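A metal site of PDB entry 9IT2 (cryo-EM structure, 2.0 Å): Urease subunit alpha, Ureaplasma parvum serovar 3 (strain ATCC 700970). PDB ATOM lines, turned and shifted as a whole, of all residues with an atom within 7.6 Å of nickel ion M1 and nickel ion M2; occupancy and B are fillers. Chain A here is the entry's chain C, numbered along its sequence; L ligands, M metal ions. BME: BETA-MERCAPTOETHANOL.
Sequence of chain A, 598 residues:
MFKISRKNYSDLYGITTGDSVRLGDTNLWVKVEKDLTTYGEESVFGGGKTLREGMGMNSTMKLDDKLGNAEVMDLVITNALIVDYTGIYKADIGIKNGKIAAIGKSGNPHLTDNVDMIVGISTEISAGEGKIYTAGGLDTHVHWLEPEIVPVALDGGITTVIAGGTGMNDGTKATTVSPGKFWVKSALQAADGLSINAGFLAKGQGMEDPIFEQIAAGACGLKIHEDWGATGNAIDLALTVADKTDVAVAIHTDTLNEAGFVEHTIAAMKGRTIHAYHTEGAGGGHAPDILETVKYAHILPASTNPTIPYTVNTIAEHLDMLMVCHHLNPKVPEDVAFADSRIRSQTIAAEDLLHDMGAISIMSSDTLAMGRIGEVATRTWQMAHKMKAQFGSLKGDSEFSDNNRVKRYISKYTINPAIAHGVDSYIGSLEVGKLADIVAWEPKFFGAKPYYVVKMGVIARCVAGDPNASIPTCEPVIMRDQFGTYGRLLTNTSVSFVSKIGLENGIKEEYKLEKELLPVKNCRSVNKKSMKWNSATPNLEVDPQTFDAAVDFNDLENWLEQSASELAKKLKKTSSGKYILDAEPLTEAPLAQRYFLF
A ring nitrogen (ND1) of His 252 sits close to a ring nitrogen (NE2) of His 225 (3.2 Å). The backbone NH (N) of His 252 is in hydrogen-bond range of the backbone carbonyl oxygen (O) of Ile 224 (2.5 Å). The backbone NH (N) of Glu 226 sits at hydrogen-bond distance from the backbone carbonyl oxygen (O) of His 252, at 3.1 Å. A ring nitrogen (ND1) of His 143 lies within hydrogen-bond range of the backbone carbonyl oxygen (O) of Thr 175, at 3.3 Å. A ring nitrogen (ND1) of His 143 is in hydrogen-bond range of the backbone carbonyl oxygen of Thr 172. The backbone carbonyl oxygen (O) of Asp 366 lies within hydrogen-bond range of the backbone NH (N) of Gly 371, at 2.8 Å. OG1 of Thr 176 lies within hydrogen-bond range of NZ of KCX 223. The backbone carbonyl oxygen of Ala 174 is in hydrogen-bond range of a ring nitrogen (NE2) of His 225, at 3.2 Å.
Thr 176 touches nickel ion M1 (CG2 to NI, 3.7 Å). Of the 28 residues printed, 5 come within 4 Å of nickel ion M1.
NE2 of His 225 touches nickel ion M2, at 3.5 Å. Of the 28 residues printed, 5 come within 4 Å of nickel ion M2. The nearest printed residue that does not touch nickel ion M2 is Asp 366 (4.1 Å).
NE2 of His 141 binds nickel ion M1 (2.0 Å). Nickel ion M1 is bound by NE2 of His 143. OD1 of Asp 366 is bound to nickel ion M1 (2.0 Å). OQ1 of KCX 223 is bound to nickel ion M1 (2.0 Å). Nickel ion M1 is bound by a sulfur (S2) of the ligand, 2.6 Å away.
Nickel ion M2 is bound by NE2 of His 278, ND1 of His 252, OQ2 of KCX 223 and S2 of the ligand. Nickel ion M2 has four donor atoms within binding distance.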
ATOM      1  N   HIS A 141     -24.049   6.760 -26.001  1.00  0.00           N
ATOM      2  CA  HIS A 141     -25.048   7.800 -26.254  1.00  0.00           C
ATOM      3  C   HIS A 141     -25.664   7.492 -27.614  1.00  0.00           C
ATOM      4  O   HIS A 141     -25.206   7.998 -28.644  1.00  0.00           O
ATOM      5  CB  HIS A 141     -24.422   9.195 -26.216  1.00  0.00           C
ATOM      6  CG  HIS A 141     -25.422  10.308 -26.230  1.00  0.00           C
ATOM      7  ND1 HIS A 141     -25.148  11.564 -25.734  1.00  0.00           N
ATOM      8  CD2 HIS A 141     -26.708  10.357 -26.677  1.00  0.00           C
ATOM      9  CE1 HIS A 141     -26.211  12.341 -25.871  1.00  0.00           C
ATOM     10  NE2 HIS A 141     -27.168  11.633 -26.442  1.00  0.00           N
ATOM     11  N   VAL A 142     -26.706   6.674 -27.619  1.00  0.00           N
ATOM     12  CA  VAL A 142     -27.349   6.222 -28.848  1.00  0.00           C
ATOM     13  C   VAL A 142     -28.855   6.445 -28.707  1.00  0.00           C
ATOM     14  O   VAL A 142     -29.473   5.950 -27.755  1.00  0.00           O
ATOM     15  CB  VAL A 142     -27.057   4.742 -29.144  1.00  0.00           C
ATOM     16  CG1 VAL A 142     -27.877   4.263 -30.343  1.00  0.00           C
ATOM     17  CG2 VAL A 142     -25.575   4.531 -29.390  1.00  0.00           C
ATOM     18  N   HIS A 143     -29.431   7.194 -29.640  1.00  0.00           N
ATOM     19  CA  HIS A 143     -30.884   7.292 -29.719  1.00  0.00           C
ATOM     20  C   HIS A 143     -31.418   6.100 -30.499  1.00  0.00           C
ATOM     21  O   HIS A 143     -30.989   5.829 -31.621  1.00  0.00           O
ATOM     22  CB  HIS A 143     -31.301   8.605 -30.385  1.00  0.00           C
ATOM     23  CG  HIS A 143     -30.970   9.825 -29.579  1.00  0.00           C
ATOM     24  ND1 HIS A 143     -31.922  10.609 -28.973  1.00  0.00           N
ATOM     25  CD2 HIS A 143     -29.771  10.401 -29.280  1.00  0.00           C
ATOM     26  CE1 HIS A 143     -31.339  11.603 -28.337  1.00  0.00           C
ATOM     27  NE2 HIS A 143     -30.040  11.505 -28.500  1.00  0.00           N
ATOM     28  N   THR A 172     -38.075  10.159 -28.587  1.00  0.00           N
ATOM     29  CA  THR A 172     -36.806   9.485 -28.886  1.00  0.00           C
ATOM     30  C   THR A 172     -35.917  10.357 -29.751  1.00  0.00           C
ATOM     31  O   THR A 172     -34.692  10.356 -29.592  1.00  0.00           O
ATOM     32  CB  THR A 172     -37.073   8.143 -29.550  1.00  0.00           C
ATOM     33  OG1 THR A 172     -37.795   7.294 -28.644  1.00  0.00           O
ATOM     34  CG2 THR A 172     -35.765   7.468 -29.952  1.00  0.00           C
ATOM     35  N   LYS A 173     -36.507  11.104 -30.690  1.00  0.00           N
ATOM     36  CA  LYS A 173     -35.724  12.007 -31.518  1.00  0.00           C
ATOM     37  C   LYS A 173     -34.993  13.052 -30.670  1.00  0.00           C
ATOM     38  O   LYS A 173     -33.921  13.528 -31.058  1.00  0.00           O
ATOM     39  CB  LYS A 173     -36.617  12.700 -32.547  1.00  0.00           C
ATOM     40  CG  LYS A 173     -37.198  11.755 -33.590  1.00  0.00           C
ATOM     41  CD  LYS A 173     -38.061  12.498 -34.596  1.00  0.00           C
ATOM     42  CE  LYS A 173     -38.826  11.518 -35.486  1.00  0.00           C
ATOM     43  NZ  LYS A 173     -39.722  12.219 -36.445  1.00  0.00           N
ATOM     44  N   ALA A 174     -35.564  13.415 -29.518  1.00  0.00           N
ATOM     45  CA  ALA A 174     -34.954  14.408 -28.650  1.00  0.00           C
ATOM     46  C   ALA A 174     -34.044  13.783 -27.590  1.00  0.00           C
ATOM     47  O   ALA A 174     -32.955  14.312 -27.328  1.00  0.00           O
ATOM     48  CB  ALA A 174     -36.033  15.247 -27.971  1.00  0.00           C
ATOM     49  N   THR A 175     -34.462  12.674 -26.978  1.00  0.00           N
ATOM     50  CA  THR A 175     -33.787  12.128 -25.814  1.00  0.00           C
ATOM     51  C   THR A 175     -33.551  10.636 -25.970  1.00  0.00           C
ATOM     52  O   THR A 175     -34.271   9.957 -26.706  1.00  0.00           O
ATOM     53  CB  THR A 175     -34.596  12.364 -24.522  1.00  0.00           C
ATOM     54  OG1 THR A 175     -35.566  11.315 -24.374  1.00  0.00           O
ATOM     55  CG2 THR A 175     -35.331  13.698 -24.570  1.00  0.00           C
ATOM     56  N   THR A 176     -32.541  10.123 -25.271  1.00  0.00           N
ATOM     57  CA  THR A 176     -32.268   8.689 -25.198  1.00  0.00           C
ATOM     58  C   THR A 176     -33.006   8.099 -23.997  1.00  0.00           C
ATOM     59  O   THR A 176     -32.418   7.779 -22.956  1.00  0.00           O
ATOM     60  CB  THR A 176     -30.781   8.409 -25.115  1.00  0.00           C
ATOM     61  OG1 THR A 176     -30.267   8.895 -23.868  1.00  0.00           O
ATOM     62  CG2 THR A 176     -30.040   9.095 -26.242  1.00  0.00           C
ATOM     63  N   KCX A 223     -31.504   8.124 -17.887  1.00  0.00           N
ATOM     64  CA  KCX A 223     -31.082   9.329 -18.582  1.00  0.00           C
ATOM     65  CB  KCX A 223     -31.169   9.151 -20.101  1.00  0.00           C
ATOM     66  CG  KCX A 223     -31.074  10.443 -20.905  1.00  0.00           C
ATOM     67  CD  KCX A 223     -29.681  11.063 -20.867  1.00  0.00           C
ATOM     68  CE  KCX A 223     -29.574  12.253 -21.810  1.00  0.00           C
ATOM     69  NZ  KCX A 223     -29.779  11.882 -23.246  1.00  0.00           N
ATOM     70  C   KCX A 223     -31.924  10.524 -18.146  1.00  0.00           C
ATOM     71  O   KCX A 223     -33.144  10.505 -18.226  1.00  0.00           O
ATOM     72  CX  KCX A 223     -29.276  12.602 -24.240  1.00  0.00           C
ATOM     73  OQ1 KCX A 223     -29.455  12.266 -25.417  1.00  0.00           O
ATOM     74  OQ2 KCX A 223     -28.609  13.625 -23.996  1.00  0.00           O
ATOM     75  N   ILE A 224     -31.249  11.555 -17.683  1.00  0.00           N
ATOM     76  CA  ILE A 224     -31.919  12.794 -17.307  1.00  0.00           C
ATOM     77  C   ILE A 224     -31.738  13.828 -18.406  1.00  0.00           C
ATOM     78  O   ILE A 224     -30.660  14.388 -18.571  1.00  0.00           O
ATOM     79  CB  ILE A 224     -31.400  13.336 -15.963  1.00  0.00           C
ATOM     80  CG1 ILE A 224     -31.501  12.262 -14.877  1.00  0.00           C
ATOM     81  CG2 ILE A 224     -32.164  14.590 -15.558  1.00  0.00           C
ATOM     82  CD1 ILE A 224     -30.729  12.593 -13.625  1.00  0.00           C
ATOM     83  N   HIS A 225     -32.807  14.066 -19.165  1.00  0.00           N
ATOM     84  CA  HIS A 225     -32.788  15.022 -20.267  1.00  0.00           C
ATOM     85  C   HIS A 225     -33.622  16.238 -19.903  1.00  0.00           C
ATOM     86  O   HIS A 225     -34.660  16.111 -19.249  1.00  0.00           O
ATOM     87  CB  HIS A 225     -33.322  14.387 -21.556  1.00  0.00           C
ATOM     88  CG  HIS A 225     -32.751  14.972 -22.798  1.00  0.00           C
ATOM     89  ND1 HIS A 225     -33.153  16.193 -23.305  1.00  0.00           N
ATOM     90  CD2 HIS A 225     -31.818  14.501 -23.658  1.00  0.00           C
ATOM     91  CE1 HIS A 225     -32.475  16.450 -24.416  1.00  0.00           C
ATOM     92  NE2 HIS A 225     -31.660  15.445 -24.652  1.00  0.00           N
ATOM     93  N   GLU A 226     -33.150  17.418 -20.310  1.00  0.00           N
ATOM     94  CA  GLU A 226     -33.863  18.649 -20.008  1.00  0.00           C
ATOM     95  C   GLU A 226     -35.202  18.718 -20.735  1.00  0.00           C
ATOM     96  O   GLU A 226     -36.125  19.390 -20.269  1.00  0.00           O
ATOM     97  CB  GLU A 226     -33.007  19.866 -20.359  1.00  0.00           C
ATOM     98  CG  GLU A 226     -32.686  20.007 -21.837  1.00  0.00           C
ATOM     99  CD  GLU A 226     -32.121  21.360 -22.181  1.00  0.00           C
ATOM    100  OE1 GLU A 226     -32.402  22.328 -21.445  1.00  0.00           O
ATOM    101  OE2 GLU A 226     -31.407  21.467 -23.196  1.00  0.00           O
ATOM    102  N   ILE A 251     -26.855  12.386 -17.876  1.00  0.00           N
ATOM    103  CA  ILE A 251     -27.586  13.645 -17.744  1.00  0.00           C
ATOM    104  C   ILE A 251     -27.395  14.495 -18.992  1.00  0.00           C
ATOM    105  O   ILE A 251     -26.297  14.556 -19.556  1.00  0.00           O
ATOM    106  CB  ILE A 251     -27.161  14.414 -16.472  1.00  0.00           C
ATOM    107  CG1 ILE A 251     -28.018  15.673 -16.308  1.00  0.00           C
ATOM    108  CG2 ILE A 251     -25.679  14.756 -16.494  1.00  0.00           C
ATOM    109  CD1 ILE A 251     -28.348  16.000 -14.871  1.00  0.00           C
ATOM    110  N   HIS A 252     -28.469  15.127 -19.427  1.00  0.00           N
ATOM    111  CA  HIS A 252     -28.457  16.214 -20.392  1.00  0.00           C
ATOM    112  C   HIS A 252     -28.961  17.436 -19.625  1.00  0.00           C
ATOM    113  O   HIS A 252     -30.169  17.634 -19.495  1.00  0.00           O
ATOM    114  CB  HIS A 252     -29.333  15.881 -21.606  1.00  0.00           C
ATOM    115  CG  HIS A 252     -29.360  16.950 -22.652  1.00  0.00           C
ATOM    116  ND1 HIS A 252     -28.874  16.753 -23.931  1.00  0.00           N
ATOM    117  CD2 HIS A 252     -29.822  18.225 -22.616  1.00  0.00           C
ATOM    118  CE1 HIS A 252     -29.033  17.857 -24.633  1.00  0.00           C
ATOM    119  NE2 HIS A 252     -29.598  18.771 -23.861  1.00  0.00           N
ATOM    120  N   THR A 253     -28.023  18.238 -19.119  1.00  0.00           N
ATOM    121  CA  THR A 253     -28.355  19.229 -18.109  1.00  0.00           C
ATOM    122  C   THR A 253     -29.174  20.378 -18.696  1.00  0.00           C
ATOM    123  O   THR A 253     -29.303  20.533 -19.913  1.00  0.00           O
ATOM    124  CB  THR A 253     -27.073  19.767 -17.453  1.00  0.00           C
ATOM    125  OG1 THR A 253     -26.433  20.690 -18.333  1.00  0.00           O
ATOM    126  CG2 THR A 253     -26.112  18.633 -17.128  1.00  0.00           C
ATOM    127  N   TYR A 277     -23.252  13.648 -20.361  1.00  0.00           N
ATOM    128  CA  TYR A 277     -23.376  13.557 -21.803  1.00  0.00           C
ATOM    129  C   TYR A 277     -22.981  14.870 -22.464  1.00  0.00           C
ATOM    130  O   TYR A 277     -23.404  15.948 -22.025  1.00  0.00           O
ATOM    131  CB  TYR A 277     -24.813  13.199 -22.197  1.00  0.00           C
ATOM    132  CG  TYR A 277     -25.099  11.718 -22.291  1.00  0.00           C
ATOM    133  CD1 TYR A 277     -24.136  10.782 -21.933  1.00  0.00           C
ATOM    134  CD2 TYR A 277     -26.328  11.267 -22.743  1.00  0.00           C
ATOM    135  CE1 TYR A 277     -24.405   9.431 -22.027  1.00  0.00           C
ATOM    136  CE2 TYR A 277     -26.597   9.915 -22.837  1.00  0.00           C
ATOM    137  CZ  TYR A 277     -25.632   9.004 -22.473  1.00  0.00           C
ATOM    138  OH  TYR A 277     -25.897   7.658 -22.561  1.00  0.00           O
ATOM    139  N   HIS A 278     -22.189  14.780 -23.534  1.00  0.00           N
ATOM    140  CA  HIS A 278     -21.748  15.912 -24.356  1.00  0.00           C
ATOM    141  C   HIS A 278     -21.415  17.128 -23.501  1.00  0.00           C
ATOM    142  O   HIS A 278     -22.034  18.187 -23.583  1.00  0.00           O
ATOM    143  CB  HIS A 278     -22.775  16.260 -25.436  1.00  0.00           C
ATOM    144  CG  HIS A 278     -24.199  16.269 -24.980  1.00  0.00           C
ATOM    145  ND1 HIS A 278     -24.625  16.964 -23.863  1.00  0.00           N
ATOM    146  CD2 HIS A 278     -25.299  15.666 -25.487  1.00  0.00           C
ATOM    147  CE1 HIS A 278     -25.921  16.790 -23.710  1.00  0.00           C
ATOM    148  NE2 HIS A 278     -26.360  16.001 -24.673  1.00  0.00           N
ATOM    149  N   GLY A 283     -24.749  20.739 -28.252  1.00  0.00           N
ATOM    150  CA  GLY A 283     -26.108  20.274 -28.436  1.00  0.00           C
ATOM    151  C   GLY A 283     -27.012  20.416 -27.237  1.00  0.00           C
ATOM    152  O   GLY A 283     -28.238  20.256 -27.375  1.00  0.00           O
ATOM    153  N   GLY A 284     -26.474  20.734 -26.070  1.00  0.00           N
ATOM    154  CA  GLY A 284     -27.268  20.887 -24.875  1.00  0.00           C
ATOM    155  C   GLY A 284     -26.414  20.901 -23.624  1.00  0.00           C
ATOM    156  O   GLY A 284     -25.273  20.434 -23.629  1.00  0.00           O
ATOM    157  N   GLY A 285     -26.957  21.439 -22.539  1.00  0.00           N
ATOM    158  CA  GLY A 285     -26.193  21.600 -21.315  1.00  0.00           C
ATOM    159  C   GLY A 285     -26.149  23.042 -20.856  1.00  0.00           C
ATOM    160  O   GLY A 285     -26.390  23.955 -21.655  1.00  0.00           O
ATOM    161  N   THR A 304     -19.630  14.069 -27.509  1.00  0.00           N
ATOM    162  CA  THR A 304     -20.214  13.519 -28.725  1.00  0.00           C
ATOM    163  C   THR A 304     -19.387  13.944 -29.928  1.00  0.00           C
ATOM    164  O   THR A 304     -18.808  15.024 -29.949  1.00  0.00           O
ATOM    165  CB  THR A 304     -21.670  13.963 -28.883  1.00  0.00           C
ATOM    166  OG1 THR A 304     -21.742  15.390 -28.846  1.00  0.00           O
ATOM    167  CG2 THR A 304     -22.520  13.388 -27.764  1.00  0.00           C
ATOM    168  N   SER A 365     -21.465   9.218 -29.533  1.00  0.00           N
ATOM    169  CA  SER A 365     -21.970   9.671 -30.822  1.00  0.00           C
ATOM    170  C   SER A 365     -23.166  10.612 -30.726  1.00  0.00           C
ATOM    171  O   SER A 365     -23.207  11.604 -31.469  1.00  0.00           O
ATOM    172  CB  SER A 365     -22.367   8.466 -31.693  1.00  0.00           C
ATOM    173  OG  SER A 365     -23.631   7.960 -31.308  1.00  0.00           O
ATOM    174  N   ASP A 366     -24.129  10.349 -29.846  1.00  0.00           N
ATOM    175  CA  ASP A 366     -25.450  10.972 -29.895  1.00  0.00           C
ATOM    176  C   ASP A 366     -26.141  10.628 -31.218  1.00  0.00           C
ATOM    177  O   ASP A 366     -26.430  11.483 -32.053  1.00  0.00           O
ATOM    178  CB  ASP A 366     -25.376  12.494 -29.691  1.00  0.00           C
ATOM    179  CG  ASP A 366     -26.621  13.072 -29.063  1.00  0.00           C
ATOM    180  OD1 ASP A 366     -27.617  12.334 -28.898  1.00  0.00           O
ATOM    181  OD2 ASP A 366     -26.617  14.280 -28.732  1.00  0.00           O
ATOM    182  N   THR A 367     -26.397   9.327 -31.387  1.00  0.00           N
ATOM    183  CA  THR A 367     -26.819   8.784 -32.668  1.00  0.00           C
ATOM    184  C   THR A 367     -28.109   9.412 -33.161  1.00  0.00           C
ATOM    185  O   THR A 367     -29.126   9.433 -32.451  1.00  0.00           O
ATOM    186  CB  THR A 367     -26.996   7.269 -32.550  1.00  0.00           C
ATOM    187  OG1 THR A 367     -25.724   6.656 -32.276  1.00  0.00           O
ATOM    188  CG2 THR A 367     -27.570   6.683 -33.830  1.00  0.00           C
ATOM    189  N   LEU A 368     -28.078   9.923 -34.387  1.00  0.00           N
ATOM    190  CA  LEU A 368     -29.230  10.415 -35.128  1.00  0.00           C
ATOM    191  C   LEU A 368     -29.993  11.534 -34.419  1.00  0.00           C
ATOM    192  O   LEU A 368     -31.127  11.838 -34.798  1.00  0.00           O
ATOM    193  CB  LEU A 368     -30.193   9.273 -35.482  1.00  0.00           C
ATOM    194  CG  LEU A 368     -29.861   8.471 -36.742  1.00  0.00           C
ATOM    195  CD1 LEU A 368     -30.690   7.208 -36.797  1.00  0.00           C
ATOM    196  CD2 LEU A 368     -30.059   9.308 -37.990  1.00  0.00           C
ATOM    197  N   ALA A 369     -29.400  12.143 -33.390  1.00  0.00           N
ATOM    198  CA  ALA A 369     -29.940  13.360 -32.797  1.00  0.00           C
ATOM    199  C   ALA A 369     -29.002  14.539 -32.976  1.00  0.00           C
ATOM    200  O   ALA A 369     -29.445  15.633 -33.346  1.00  0.00           O
ATOM    201  CB  ALA A 369     -30.249  13.139 -31.310  1.00  0.00           C
ATOM    202  N   MET A 370     -27.708  14.345 -32.716  1.00  0.00           N
ATOM    203  CA  MET A 370     -26.695  15.333 -33.078  1.00  0.00           C
ATOM    204  C   MET A 370     -25.460  14.741 -33.733  1.00  0.00           C
ATOM    205  O   MET A 370     -24.736  15.488 -34.414  1.00  0.00           O
ATOM    206  CB  MET A 370     -26.273  16.141 -31.844  1.00  0.00           C
ATOM    207  CG  MET A 370     -25.493  17.404 -32.176  1.00  0.00           C
ATOM    208  SD  MET A 370     -26.487  18.910 -32.059  1.00  0.00           S
ATOM    209  CE  MET A 370     -25.196  20.135 -31.859  1.00  0.00           C
ATOM    210  N   GLY A 371     -25.175  13.457 -33.568  1.00  0.00           N
ATOM    211  CA  GLY A 371     -23.934  12.900 -34.075  1.00  0.00           C
ATOM    212  C   GLY A 371     -24.073  11.634 -34.896  1.00  0.00           C
ATOM    213  O   GLY A 371     -25.184  11.238 -35.261  1.00  0.00           O
HETATM  214  C1  BME L   1     -28.608  16.895 -28.382  1.00  0.00           C
HETATM  215  C2  BME L   1     -29.545  15.703 -28.593  1.00  0.00           C
HETATM  216  O1  BME L   1     -27.504  16.475 -27.603  1.00  0.00           O
HETATM  217  S2  BME L   1     -29.737  14.817 -27.030  1.00  0.00           S
HETATM  218 NI    NI M   1     -28.769  12.422 -27.284  1.00  0.00          NI
HETATM  219 NI    NI M   2     -28.160  15.274 -25.026  1.00  0.00          NI
